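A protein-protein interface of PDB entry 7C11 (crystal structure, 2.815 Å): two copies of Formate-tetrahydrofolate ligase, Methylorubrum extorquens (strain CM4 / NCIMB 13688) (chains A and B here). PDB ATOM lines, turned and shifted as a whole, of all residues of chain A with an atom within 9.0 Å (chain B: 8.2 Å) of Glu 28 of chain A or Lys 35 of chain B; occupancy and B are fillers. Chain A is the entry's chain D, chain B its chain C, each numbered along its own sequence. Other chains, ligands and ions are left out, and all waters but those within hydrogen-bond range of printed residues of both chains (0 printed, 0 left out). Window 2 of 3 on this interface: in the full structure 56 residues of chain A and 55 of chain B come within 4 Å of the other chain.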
ATOM      1  N   ALA A  17      19.475  -7.463   4.939  1.00  0.00           N
ATOM      2  CA  ALA A  17      19.201  -6.561   6.075  1.00  0.00           C
ATOM      3  C   ALA A  17      19.962  -5.236   5.855  1.00  0.00           C
ATOM      4  O   ALA A  17      19.389  -4.157   6.091  1.00  0.00           O
ATOM      5  CB  ALA A  17      19.534  -7.237   7.375  1.00  0.00           C
ATOM      6  N   ALA A  20      18.159  -3.169   3.344  1.00  0.00           N
ATOM      7  CA  ALA A  20      16.833  -2.823   3.873  1.00  0.00           C
ATOM      8  C   ALA A  20      16.919  -1.554   4.726  1.00  0.00           C
ATOM      9  O   ALA A  20      16.006  -0.737   4.615  1.00  0.00           O
ATOM     10  CB  ALA A  20      16.323  -4.011   4.631  1.00  0.00           C
ATOM     11  N   GLY A  24      14.735   2.296   5.828  1.00  0.00           N
ATOM     12  CA  GLY A  24      14.065   2.356   7.142  1.00  0.00           C
ATOM     13  C   GLY A  24      13.456   1.012   7.510  1.00  0.00           C
ATOM     14  O   GLY A  24      12.672   0.947   8.470  1.00  0.00           O
ATOM     15  N   ILE A  25      13.794  -0.047   6.782  1.00  0.00           N
ATOM     16  CA  ILE A  25      13.172  -1.372   6.996  1.00  0.00           C
ATOM     17  C   ILE A  25      14.008  -2.072   8.064  1.00  0.00           C
ATOM     18  O   ILE A  25      15.183  -2.367   7.856  1.00  0.00           O
ATOM     19  CB  ILE A  25      13.031  -2.141   5.661  1.00  0.00           C
ATOM     20  CG1 ILE A  25      12.406  -1.268   4.567  1.00  0.00           C
ATOM     21  CG2 ILE A  25      12.245  -3.433   5.842  1.00  0.00           C
ATOM     22  CD1 ILE A  25      12.634  -1.783   3.153  1.00  0.00           C
ATOM     23  N   PRO A  26      13.432  -2.342   9.260  1.00  0.00           N
ATOM     24  CA  PRO A  26      14.114  -3.165  10.259  1.00  0.00           C
ATOM     25  C   PRO A  26      14.121  -4.639   9.824  1.00  0.00           C
ATOM     26  O   PRO A  26      13.232  -5.012   9.070  1.00  0.00           O
ATOM     27  CB  PRO A  26      13.260  -2.924  11.509  1.00  0.00           C
ATOM     28  CG  PRO A  26      11.866  -2.669  10.978  1.00  0.00           C
ATOM     29  CD  PRO A  26      12.090  -1.912   9.692  1.00  0.00           C
ATOM     30  N   ASP A  27      15.092  -5.423  10.320  1.00  0.00           N
ATOM     31  CA  ASP A  27      15.294  -6.873  10.021  1.00  0.00           C
ATOM     32  C   ASP A  27      14.025  -7.641  10.410  1.00  0.00           C
ATOM     33  O   ASP A  27      13.653  -8.547   9.667  1.00  0.00           O
ATOM     34  CB  ASP A  27      16.548  -7.427  10.724  1.00  0.00           C
ATOM     35  CG  ASP A  27      16.931  -8.873  10.390  1.00  0.00           C
ATOM     36  OD1 ASP A  27      16.746  -9.313   9.217  1.00  0.00           O
ATOM     37  OD2 ASP A  27      17.427  -9.564  11.307  1.00  0.00           O
ATOM     38  N   GLU A  28      13.382  -7.243  11.512  1.00  0.00           N
ATOM     39  CA  GLU A  28      12.115  -7.814  12.049  1.00  0.00           C
ATOM     40  C   GLU A  28      11.043  -7.825  10.952  1.00  0.00           C
ATOM     41  O   GLU A  28      10.105  -8.651  11.058  1.00  0.00           O
ATOM     42  CB  GLU A  28      11.602  -6.990  13.243  1.00  0.00           C
ATOM     43  CG  GLU A  28      12.440  -7.111  14.517  1.00  0.00           C
ATOM     44  CD  GLU A  28      13.715  -6.266  14.605  1.00  0.00           C
ATOM     45  OE1 GLU A  28      14.522  -6.503  15.535  1.00  0.00           O
ATOM     46  OE2 GLU A  28      13.903  -5.358  13.750  1.00  0.00           O
ATOM     47  N   ALA A  29      11.148  -6.908   9.975  1.00  0.00           N
ATOM     48  CA  ALA A  29      10.165  -6.703   8.884  1.00  0.00           C
ATOM     49  C   ALA A  29      10.490  -7.535   7.638  1.00  0.00           C
ATOM     50  O   ALA A  29       9.704  -7.480   6.692  1.00  0.00           O
ATOM     51  CB  ALA A  29      10.104  -5.246   8.520  1.00  0.00           C
ATOM     52  N   LEU A  30      11.601  -8.259   7.614  1.00  0.00           N
ATOM     53  CA  LEU A  30      12.002  -9.047   6.422  1.00  0.00           C
ATOM     54  C   LEU A  30      11.757 -10.555   6.627  1.00  0.00           C
ATOM     55  O   LEU A  30      12.083 -11.082   7.683  1.00  0.00           O
ATOM     56  CB  LEU A  30      13.472  -8.740   6.125  1.00  0.00           C
ATOM     57  CG  LEU A  30      13.790  -7.282   5.804  1.00  0.00           C
ATOM     58  CD1 LEU A  30      15.245  -7.138   5.360  1.00  0.00           C
ATOM     59  CD2 LEU A  30      12.843  -6.726   4.743  1.00  0.00           C
ATOM     60  N   HIS A  31      11.189 -11.216   5.628  1.00  0.00           N
ATOM     61  CA  HIS A  31      11.139 -12.694   5.481  1.00  0.00           C
ATOM     62  C   HIS A  31      12.186 -13.116   4.441  1.00  0.00           C
ATOM     63  O   HIS A  31      11.881 -13.035   3.214  1.00  0.00           O
ATOM     64  CB  HIS A  31       9.736 -13.125   5.057  1.00  0.00           C
ATOM     65  CG  HIS A  31       8.665 -12.627   5.953  1.00  0.00           C
ATOM     66  ND1 HIS A  31       8.345 -13.269   7.133  1.00  0.00           N
ATOM     67  CD2 HIS A  31       7.813 -11.594   5.837  1.00  0.00           C
ATOM     68  CE1 HIS A  31       7.341 -12.630   7.720  1.00  0.00           C
ATOM     69  NE2 HIS A  31       7.006 -11.604   6.953  1.00  0.00           N
ATOM     70  N   ASN A  32      13.377 -13.503   4.921  1.00  0.00           N
ATOM     71  CA  ASN A  32      14.557 -13.876   4.092  1.00  0.00           C
ATOM     72  C   ASN A  32      14.138 -14.971   3.105  1.00  0.00           C
ATOM     73  O   ASN A  32      13.336 -15.862   3.461  1.00  0.00           O
ATOM     74  CB  ASN A  32      15.775 -14.294   4.937  1.00  0.00           C
ATOM     75  CG  ASN A  32      16.598 -13.108   5.423  1.00  0.00           C
ATOM     76  OD1 ASN A  32      16.084 -12.205   6.081  1.00  0.00           O
ATOM     77  ND2 ASN A  32      17.878 -13.068   5.081  1.00  0.00           N
ATOM     78  N   TYR A  33      14.643 -14.864   1.884  1.00  0.00           N
ATOM     79  CA  TYR A  33      14.730 -15.958   0.892  1.00  0.00           C
ATOM     80  C   TYR A  33      16.200 -16.146   0.528  1.00  0.00           C
ATOM     81  O   TYR A  33      16.654 -15.373  -0.321  1.00  0.00           O
ATOM     82  CB  TYR A  33      13.893 -15.558  -0.315  1.00  0.00           C
ATOM     83  CG  TYR A  33      12.442 -15.909  -0.162  1.00  0.00           C
ATOM     84  CD1 TYR A  33      11.587 -15.086   0.549  1.00  0.00           C
ATOM     85  CD2 TYR A  33      11.950 -17.084  -0.704  1.00  0.00           C
ATOM     86  CE1 TYR A  33      10.254 -15.422   0.703  1.00  0.00           C
ATOM     87  CE2 TYR A  33      10.622 -17.432  -0.563  1.00  0.00           C
ATOM     88  CZ  TYR A  33       9.772 -16.596   0.138  1.00  0.00           C
ATOM     89  OH  TYR A  33       8.460 -16.952   0.271  1.00  0.00           O
ATOM     90  N   GLY A  34      16.924 -17.060   1.183  1.00  0.00           N
ATOM     91  CA  GLY A  34      18.403 -17.012   1.219  1.00  0.00           C
ATOM     92  C   GLY A  34      18.898 -15.786   1.991  1.00  0.00           C
ATOM     93  O   GLY A  34      18.132 -15.261   2.820  1.00  0.00           O
ATOM     94  N   LYS A  39      11.159 -10.721   1.507  1.00  0.00           N
ATOM     95  CA  LYS A  39       9.878 -10.018   1.269  1.00  0.00           C
ATOM     96  C   LYS A  39       9.725  -9.030   2.420  1.00  0.00           C
ATOM     97  O   LYS A  39      10.314  -9.301   3.473  1.00  0.00           O
ATOM     98  CB  LYS A  39       8.721 -11.011   1.116  1.00  0.00           C
ATOM     99  CG  LYS A  39       8.810 -11.865  -0.142  1.00  0.00           C
ATOM    100  CD  LYS A  39       7.850 -13.033  -0.179  1.00  0.00           C
ATOM    101  CE  LYS A  39       6.657 -12.800  -1.077  1.00  0.00           C
ATOM    102  NZ  LYS A  39       7.037 -12.752  -2.511  1.00  0.00           N
ATOM    103  N   ILE A  40       9.034  -7.906   2.191  1.00  0.00           N
ATOM    104  CA  ILE A  40       8.694  -6.886   3.228  1.00  0.00           C
ATOM    105  C   ILE A  40       7.290  -7.194   3.734  1.00  0.00           C
ATOM    106  O   ILE A  40       6.374  -7.246   2.902  1.00  0.00           O
ATOM    107  CB  ILE A  40       8.783  -5.453   2.687  1.00  0.00           C
ATOM    108  CG1 ILE A  40      10.154  -5.185   2.068  1.00  0.00           C
ATOM    109  CG2 ILE A  40       8.432  -4.441   3.774  1.00  0.00           C
ATOM    110  CD1 ILE A  40      10.116  -4.262   0.881  1.00  0.00           C
ATOM    111  N   ASP A  41       7.164  -7.396   5.045  1.00  0.00           N
ATOM    112  CA  ASP A  41       5.998  -8.019   5.714  1.00  0.00           C
ATOM    113  C   ASP A  41       4.806  -7.072   5.570  1.00  0.00           C
ATOM    114  O   ASP A  41       4.984  -5.870   5.750  1.00  0.00           O
ATOM    115  CB  ASP A  41       6.380  -8.350   7.160  1.00  0.00           C
ATOM    116  CG  ASP A  41       5.226  -8.324   8.128  1.00  0.00           C
ATOM    117  OD1 ASP A  41       4.446  -9.285   8.113  1.00  0.00           O
ATOM    118  OD2 ASP A  41       5.102  -7.321   8.851  1.00  0.00           O
ATOM    119  N   HIS A  42       3.639  -7.612   5.242  1.00  0.00           N
ATOM    120  CA  HIS A  42       2.343  -6.886   5.128  1.00  0.00           C
ATOM    121  C   HIS A  42       2.228  -5.769   6.179  1.00  0.00           C
ATOM    122  O   HIS A  42       1.822  -4.651   5.808  1.00  0.00           O
ATOM    123  CB  HIS A  42       1.186  -7.885   5.240  1.00  0.00           C
ATOM    124  CG  HIS A  42       1.062  -8.766   4.050  1.00  0.00           C
ATOM    125  ND1 HIS A  42       1.008  -8.258   2.768  1.00  0.00           N
ATOM    126  CD2 HIS A  42       0.970 -10.112   3.936  1.00  0.00           C
ATOM    127  CE1 HIS A  42       0.865  -9.263   1.915  1.00  0.00           C
ATOM    128  NE2 HIS A  42       0.836 -10.413   2.606  1.00  0.00           N
ATOM    129  N   ASP A  43       2.543  -6.060   7.441  1.00  0.00           N
ATOM    130  CA  ASP A  43       2.253  -5.150   8.579  1.00  0.00           C
ATOM    131  C   ASP A  43       3.100  -3.878   8.479  1.00  0.00           C
ATOM    132  O   ASP A  43       2.573  -2.806   8.886  1.00  0.00           O
ATOM    133  CB  ASP A  43       2.498  -5.827   9.926  1.00  0.00           C
ATOM    134  CG  ASP A  43       1.298  -6.607  10.417  1.00  0.00           C
ATOM    135  OD1 ASP A  43       0.587  -7.182   9.557  1.00  0.00           O
ATOM    136  OD2 ASP A  43       1.076  -6.613  11.655  1.00  0.00           O
ATOM    137  N   PHE A  44       4.364  -4.006   8.030  1.00  0.00           N
ATOM    138  CA  PHE A  44       5.319  -2.882   7.843  1.00  0.00           C
ATOM    139  C   PHE A  44       4.814  -1.993   6.707  1.00  0.00           C
ATOM    140  O   PHE A  44       4.939  -0.771   6.819  1.00  0.00           O
ATOM    141  CB  PHE A  44       6.752  -3.361   7.574  1.00  0.00           C
ATOM    142  CG  PHE A  44       7.746  -2.260   7.286  1.00  0.00           C
ATOM    143  CD1 PHE A  44       8.355  -1.555   8.315  1.00  0.00           C
ATOM    144  CD2 PHE A  44       8.058  -1.907   5.980  1.00  0.00           C
ATOM    145  CE1 PHE A  44       9.250  -0.526   8.048  1.00  0.00           C
ATOM    146  CE2 PHE A  44       8.949  -0.877   5.711  1.00  0.00           C
ATOM    147  CZ  PHE A  44       9.544  -0.184   6.746  1.00  0.00           C
ATOM    148  N   LEU B  13       7.995 -19.576  18.207  1.00  0.00           N
ATOM    149  CA  LEU B  13       8.990 -20.426  17.502  1.00  0.00           C
ATOM    150  C   LEU B  13      10.390 -19.845  17.686  1.00  0.00           C
ATOM    151  O   LEU B  13      10.530 -18.606  17.648  1.00  0.00           O
ATOM    152  CB  LEU B  13       8.627 -20.499  16.016  1.00  0.00           C
ATOM    153  CG  LEU B  13       7.694 -21.642  15.638  1.00  0.00           C
ATOM    154  CD1 LEU B  13       6.485 -21.683  16.565  1.00  0.00           C
ATOM    155  CD2 LEU B  13       7.257 -21.500  14.197  1.00  0.00           C
ATOM    156  N   LYS B  14      11.388 -20.716  17.840  1.00  0.00           N
ATOM    157  CA  LYS B  14      12.815 -20.320  17.862  1.00  0.00           C
ATOM    158  C   LYS B  14      13.186 -19.816  16.469  1.00  0.00           C
ATOM    159  O   LYS B  14      12.695 -20.328  15.466  1.00  0.00           O
ATOM    160  CB  LYS B  14      13.676 -21.484  18.367  1.00  0.00           C
ATOM    161  CG  LYS B  14      13.530 -21.782  19.859  1.00  0.00           C
ATOM    162  CD  LYS B  14      14.813 -22.210  20.584  1.00  0.00           C
ATOM    163  CE  LYS B  14      14.838 -21.821  22.058  1.00  0.00           C
ATOM    164  NZ  LYS B  14      14.682 -22.979  22.976  1.00  0.00           N
ATOM    165  N   PRO B  15      14.012 -18.747  16.347  1.00  0.00           N
ATOM    166  CA  PRO B  15      14.641 -18.425  15.068  1.00  0.00           C
ATOM    167  C   PRO B  15      15.287 -19.707  14.545  1.00  0.00           C
ATOM    168  O   PRO B  15      15.842 -20.434  15.330  1.00  0.00           O
ATOM    169  CB  PRO B  15      15.670 -17.339  15.423  1.00  0.00           C
ATOM    170  CG  PRO B  15      15.118 -16.682  16.669  1.00  0.00           C
ATOM    171  CD  PRO B  15      14.381 -17.783  17.409  1.00  0.00           C
ATOM    172  N   ILE B  16      15.177 -19.970  13.253  1.00  0.00           N
ATOM    173  CA  ILE B  16      15.573 -21.289  12.683  1.00  0.00           C
ATOM    174  C   ILE B  16      17.066 -21.597  12.948  1.00  0.00           C
ATOM    175  O   ILE B  16      17.371 -22.815  13.145  1.00  0.00           O
ATOM    176  CB  ILE B  16      15.218 -21.387  11.194  1.00  0.00           C
ATOM    177  CG1 ILE B  16      15.275 -22.847  10.760  1.00  0.00           C
ATOM    178  CG2 ILE B  16      16.113 -20.505  10.350  1.00  0.00           C
ATOM    179  CD1 ILE B  16      14.382 -23.747  11.581  1.00  0.00           C
ATOM    180  N   ALA B  17      17.963 -20.593  12.973  1.00  0.00           N
ATOM    181  CA  ALA B  17      19.419 -20.830  13.171  1.00  0.00           C
ATOM    182  C   ALA B  17      19.689 -21.458  14.544  1.00  0.00           C
ATOM    183  O   ALA B  17      20.707 -22.154  14.673  1.00  0.00           O
ATOM    184  CB  ALA B  17      20.232 -19.576  12.985  1.00  0.00           C
ATOM    185  N   GLN B  18      18.808 -21.237  15.519  1.00  0.00           N
ATOM    186  CA  GLN B  18      18.890 -21.831  16.888  1.00  0.00           C
ATOM    187  C   GLN B  18      18.577 -23.330  16.824  1.00  0.00           C
ATOM    188  O   GLN B  18      19.293 -24.099  17.468  1.00  0.00           O
ATOM    189  CB  GLN B  18      17.947 -21.121  17.869  1.00  0.00           C
ATOM    190  CG  GLN B  18      18.614 -19.971  18.614  1.00  0.00           C
ATOM    191  CD  GLN B  18      17.664 -18.872  19.029  1.00  0.00           C
ATOM    192  OE1 GLN B  18      17.801 -17.728  18.578  1.00  0.00           O
ATOM    193  NE2 GLN B  18      16.711 -19.208  19.899  1.00  0.00           N
ATOM    194  N   VAL B  19      17.529 -23.711  16.094  1.00  0.00           N
ATOM    195  CA  VAL B  19      17.101 -25.129  15.898  1.00  0.00           C
ATOM    196  C   VAL B  19      18.256 -25.851  15.206  1.00  0.00           C
ATOM    197  O   VAL B  19      18.654 -26.918  15.691  1.00  0.00           O
ATOM    198  CB  VAL B  19      15.807 -25.196  15.067  1.00  0.00           C
ATOM    199  CG1 VAL B  19      15.368 -26.627  14.801  1.00  0.00           C
ATOM    200  CG2 VAL B  19      14.695 -24.381  15.716  1.00  0.00           C
ATOM    201  N   LEU B  30      22.645 -22.112   5.862  1.00  0.00           N
ATOM    202  CA  LEU B  30      21.164 -22.003   5.906  1.00  0.00           C
ATOM    203  C   LEU B  30      20.624 -21.027   4.850  1.00  0.00           C
ATOM    204  O   LEU B  30      20.932 -19.825   4.926  1.00  0.00           O
ATOM    205  CB  LEU B  30      20.767 -21.570   7.319  1.00  0.00           C
ATOM    206  CG  LEU B  30      20.973 -22.627   8.404  1.00  0.00           C
ATOM    207  CD1 LEU B  30      20.384 -22.155   9.724  1.00  0.00           C
ATOM    208  CD2 LEU B  30      20.366 -23.972   8.014  1.00  0.00           C
ATOM    209  N   ASN B  32      17.385 -19.384   4.247  1.00  0.00           N
ATOM    210  CA  ASN B  32      16.131 -19.047   4.967  1.00  0.00           C
ATOM    211  C   ASN B  32      14.970 -18.919   3.975  1.00  0.00           C
ATOM    212  O   ASN B  32      15.190 -18.420   2.823  1.00  0.00           O
ATOM    213  CB  ASN B  32      16.250 -17.749   5.777  1.00  0.00           C
ATOM    214  CG  ASN B  32      17.269 -17.845   6.889  1.00  0.00           C
ATOM    215  OD1 ASN B  32      16.916 -18.089   8.042  1.00  0.00           O
ATOM    216  ND2 ASN B  32      18.537 -17.685   6.533  1.00  0.00           N
ATOM    217  N   TYR B  33      13.790 -19.379   4.409  1.00  0.00           N
ATOM    218  CA  TYR B  33      12.453 -19.072   3.840  1.00  0.00           C
ATOM    219  C   TYR B  33      11.659 -18.469   4.994  1.00  0.00           C
ATOM    220  O   TYR B  33      10.983 -19.195   5.762  1.00  0.00           O
ATOM    221  CB  TYR B  33      11.812 -20.319   3.234  1.00  0.00           C
ATOM    222  CG  TYR B  33      12.473 -20.789   1.965  1.00  0.00           C
ATOM    223  CD1 TYR B  33      13.714 -21.401   1.993  1.00  0.00           C
ATOM    224  CD2 TYR B  33      11.868 -20.603   0.737  1.00  0.00           C
ATOM    225  CE1 TYR B  33      14.351 -21.800   0.832  1.00  0.00           C
ATOM    226  CE2 TYR B  33      12.484 -21.006  -0.436  1.00  0.00           C
ATOM    227  CZ  TYR B  33      13.728 -21.614  -0.392  1.00  0.00           C
ATOM    228  OH  TYR B  33      14.342 -22.023  -1.546  1.00  0.00           O
ATOM    229  N   GLY B  34      11.817 -17.155   5.151  1.00  0.00           N
ATOM    230  CA  GLY B  34      11.391 -16.423   6.353  1.00  0.00           C
ATOM    231  C   GLY B  34      12.220 -16.849   7.544  1.00  0.00           C
ATOM    232  O   GLY B  34      13.354 -17.338   7.327  1.00  0.00           O
ATOM    233  N   LYS B  35      11.668 -16.717   8.751  1.00  0.00           N
ATOM    234  CA  LYS B  35      12.444 -16.885  10.003  1.00  0.00           C
ATOM    235  C   LYS B  35      12.435 -18.356  10.419  1.00  0.00           C
ATOM    236  O   LYS B  35      13.447 -18.796  10.974  1.00  0.00           O
ATOM    237  CB  LYS B  35      11.925 -15.938  11.089  1.00  0.00           C
ATOM    238  CG  LYS B  35      11.918 -14.478  10.657  1.00  0.00           C
ATOM    239  CD  LYS B  35      11.811 -13.478  11.777  1.00  0.00           C
ATOM    240  CE  LYS B  35      11.611 -12.064  11.266  1.00  0.00           C
ATOM    241  NZ  LYS B  35      11.110 -11.164  12.335  1.00  0.00           N
ATOM    242  N   HIS B  36      11.369 -19.099  10.129  1.00  0.00           N
ATOM    243  CA  HIS B  36      11.025 -20.336  10.876  1.00  0.00           C
ATOM    244  C   HIS B  36      11.327 -21.578  10.027  1.00  0.00           C
ATOM    245  O   HIS B  36      11.046 -22.715  10.503  1.00  0.00           O
ATOM    246  CB  HIS B  36       9.588 -20.197  11.401  1.00  0.00           C
ATOM    247  CG  HIS B  36       9.416 -18.980  12.252  1.00  0.00           C
ATOM    248  ND1 HIS B  36      10.323 -18.636  13.252  1.00  0.00           N
ATOM    249  CD2 HIS B  36       8.468 -18.017  12.262  1.00  0.00           C
ATOM    250  CE1 HIS B  36       9.927 -17.529  13.847  1.00  0.00           C
ATOM    251  NE2 HIS B  36       8.795 -17.123  13.256  1.00  0.00           N
ATOM    252  N   ILE B  37      11.917 -21.368   8.844  1.00  0.00           N
ATOM    253  CA  ILE B  37      12.343 -22.431   7.882  1.00  0.00           C
ATOM    254  C   ILE B  37      13.682 -22.029   7.284  1.00  0.00           C
ATOM    255  O   ILE B  37      13.802 -20.879   6.890  1.00  0.00           O
ATOM    256  CB  ILE B  37      11.341 -22.616   6.728  1.00  0.00           C
ATOM    257  CG1 ILE B  37       9.907 -22.841   7.206  1.00  0.00           C
ATOM    258  CG2 ILE B  37      11.808 -23.735   5.824  1.00  0.00           C
ATOM    259  CD1 ILE B  37       8.863 -22.456   6.164  1.00  0.00           C
ATOM    260  N   ALA B  38      14.599 -22.977   7.149  1.00  0.00           N
ATOM    261  CA  ALA B  38      15.825 -22.859   6.331  1.00  0.00           C
ATOM    262  C   ALA B  38      16.023 -24.161   5.554  1.00  0.00           C
ATOM    263  O   ALA B  38      15.598 -25.205   6.049  1.00  0.00           O
ATOM    264  CB  ALA B  38      17.019 -22.558   7.210  1.00  0.00           C
ATOM    265  N   PRO B 118       6.294 -24.087  11.053  1.00  0.00           N
ATOM    266  CA  PRO B 118       4.897 -23.621  11.022  1.00  0.00           C
ATOM    267  C   PRO B 118       3.925 -24.318  10.050  1.00  0.00           C
ATOM    268  O   PRO B 118       4.297 -24.515   8.892  1.00  0.00           O
ATOM    269  CB  PRO B 118       5.040 -22.161  10.561  1.00  0.00           C
ATOM    270  CG  PRO B 118       6.224 -22.208   9.615  1.00  0.00           C
ATOM    271  CD  PRO B 118       7.160 -23.263  10.187  1.00  0.00           C
ATOM    272  N   GLN B 121       2.471 -22.842   6.244  1.00  0.00           N
ATOM    273  CA  GLN B 121       3.481 -22.927   5.178  1.00  0.00           C
ATOM    274  C   GLN B 121       3.705 -24.408   4.814  1.00  0.00           C
ATOM    275  O   GLN B 121       3.884 -24.717   3.609  1.00  0.00           O
ATOM    276  CB  GLN B 121       4.769 -22.223   5.628  1.00  0.00           C
ATOM    277  CG  GLN B 121       4.638 -20.722   5.840  1.00  0.00           C
ATOM    278  CD  GLN B 121       4.243 -20.396   7.255  1.00  0.00           C
ATOM    279  OE1 GLN B 121       3.303 -20.965   7.783  1.00  0.00           O
ATOM    280  NE2 GLN B 121       4.961 -19.482   7.885  1.00  0.00           N
ATOM    281  N   LEU B 256      14.709 -27.611   6.823  1.00  0.00           N
ATOM    282  CA  LEU B 256      14.830 -27.667   8.300  1.00  0.00           C
ATOM    283  C   LEU B 256      13.655 -26.895   8.898  1.00  0.00           C
ATOM    284  O   LEU B 256      13.511 -25.716   8.576  1.00  0.00           O
ATOM    285  CB  LEU B 256      16.165 -27.071   8.762  1.00  0.00           C
ATOM    286  CG  LEU B 256      16.431 -27.239  10.258  1.00  0.00           C
ATOM    287  CD1 LEU B 256      16.607 -28.708  10.597  1.00  0.00           C
ATOM    288  CD2 LEU B 256      17.644 -26.443  10.725  1.00  0.00           C
ATOM    289  N   GLN B 258      11.147 -27.099  12.955  1.00  0.00           N
ATOM    290  CA  GLN B 258      11.180 -27.498  14.387  1.00  0.00           C
ATOM    291  C   GLN B 258       9.853 -28.135  14.836  1.00  0.00           C
ATOM    292  O   GLN B 258       8.844 -28.008  14.093  1.00  0.00           O
ATOM    293  CB  GLN B 258      11.470 -26.264  15.245  1.00  0.00           C
ATOM    294  CG  GLN B 258      10.507 -25.098  15.044  1.00  0.00           C
ATOM    295  CD  GLN B 258      10.992 -23.871  15.774  1.00  0.00           C
ATOM    296  OE1 GLN B 258      11.343 -22.859  15.172  1.00  0.00           O
ATOM    297  NE2 GLN B 258      11.067 -23.980  17.081  1.00  0.00           N
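Lys 35 of chain B touches Leu 30 of chain A. Gly 34 of chain B touches His 31 of chain A (CA to CA, 3.8 Å). Asn 32 of chain A touches Tyr 33 of chain B (O to CA, 3.4 Å). Tyr 33 of chain A touches Asn 32 of chain B. Tyr 33 of chain B touches Tyr 33 of chain A.
Printed residues of chain B that touch a printed residue of chain A: Asn 32, Tyr 33, Gly 34 and Lys 35. Hydrophobic or aromatic side chains of chain B that line the printed part of chain A: Tyr 33. Of the 19 printed residues of chain A, 6 touch a printed residue of chain B. Hydrophobic or aromatic side chains of chain A within 4 Å of the printed part of chain B: His 31 and Tyr 33. Among the printed residues, no Asp or Glu carboxylate lies within 4 Å of a Lys or Arg side-chain nitrogen of the other chain.
Asn 32 of chain B touches its own counterpart, Asn 32 of chain A. Asn 32 of chain A touches Tyr 33 of chain B, and with the chains exchanged Tyr 33 of chain A touches Asn 32 of chain B. Asn 32 of chain A touches Gly 34 of chain B, and with the chains exchanged Gly 34 of chain A touches Asn 32 of chain B. Tyr 33 of chain B touches its own counterpart, Tyr 33 of chain A. 5 positions are printed for both chains. Of the 9 pairs that touch across the chains among the printed residues, 6 have their exchanged pair printed and touching as well.
Of chain B, only Lys 35 comes within 4 Å of Glu 28 of chain A. Printed residues of chain B within 4 Å of Leu 30 of chain A: Lys 35 (3.7 Å). Of the printed residues of chain B, Gly 34 of chain A touches Asn 32. Asp 43 of chain A touches none of the printed residues of chain B. Printed residues of chain A within 4 Å of Asn 32 of chain B: Asn 32 (3.2 Å), Tyr 33 (3.2 Å) and Gly 34 (2.7 Å). Gly 34 of chain B touches just these residues of chain A: His 31 (3.8 Å) and Asn 32 (2.6 Å). Printed residues of chain A within 4 Å of Lys 35 of chain B: Glu 28 (3.0 Å) and Leu 30 (3.7 Å). No residue of chain A comes within 4 Å of His 36 of chain B. The nearest printed residue of chain A that does not touch Asn 32 of chain B is His 31 of chain A (6.3 Å).
The backbone NH (N) of Ile 16 of chain B lies within hydrogen-bond range of the backbone carbonyl oxygen (O) of Lys 35 of chain B, at 3.1 Å. The backbone carbonyl oxygen of His 31 of chain A lies within hydrogen-bond range of the backbone NH of Lys 39 of chain A, 3.0 Å away. The side-chain amide nitrogen (ND2) of Asn 32 of chain A lies within hydrogen-bond range of the backbone carbonyl oxygen (O) of Gly 34 of chain A (3.2 Å).
The backbone carbonyl oxygen of Asn 32 of chain B lies within hydrogen-bond range of the backbone NH of Gly 34 of chain A (2.7 Å). The backbone NH (N) of Gly 34 of chain B lies within hydrogen-bond range of the backbone carbonyl oxygen (O) of Asn 32 of chain A (2.6 Å). NZ of Lys 35 of chain B is in hydrogen-bond range of O of Glu 28 of chain A, 3.0 Å away. The backbone carbonyl oxygen (O) of Asn 32 of chain B sits close to the backbone carbonyl oxygen (O) of Asn 32 of chain A (3.2 Å).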
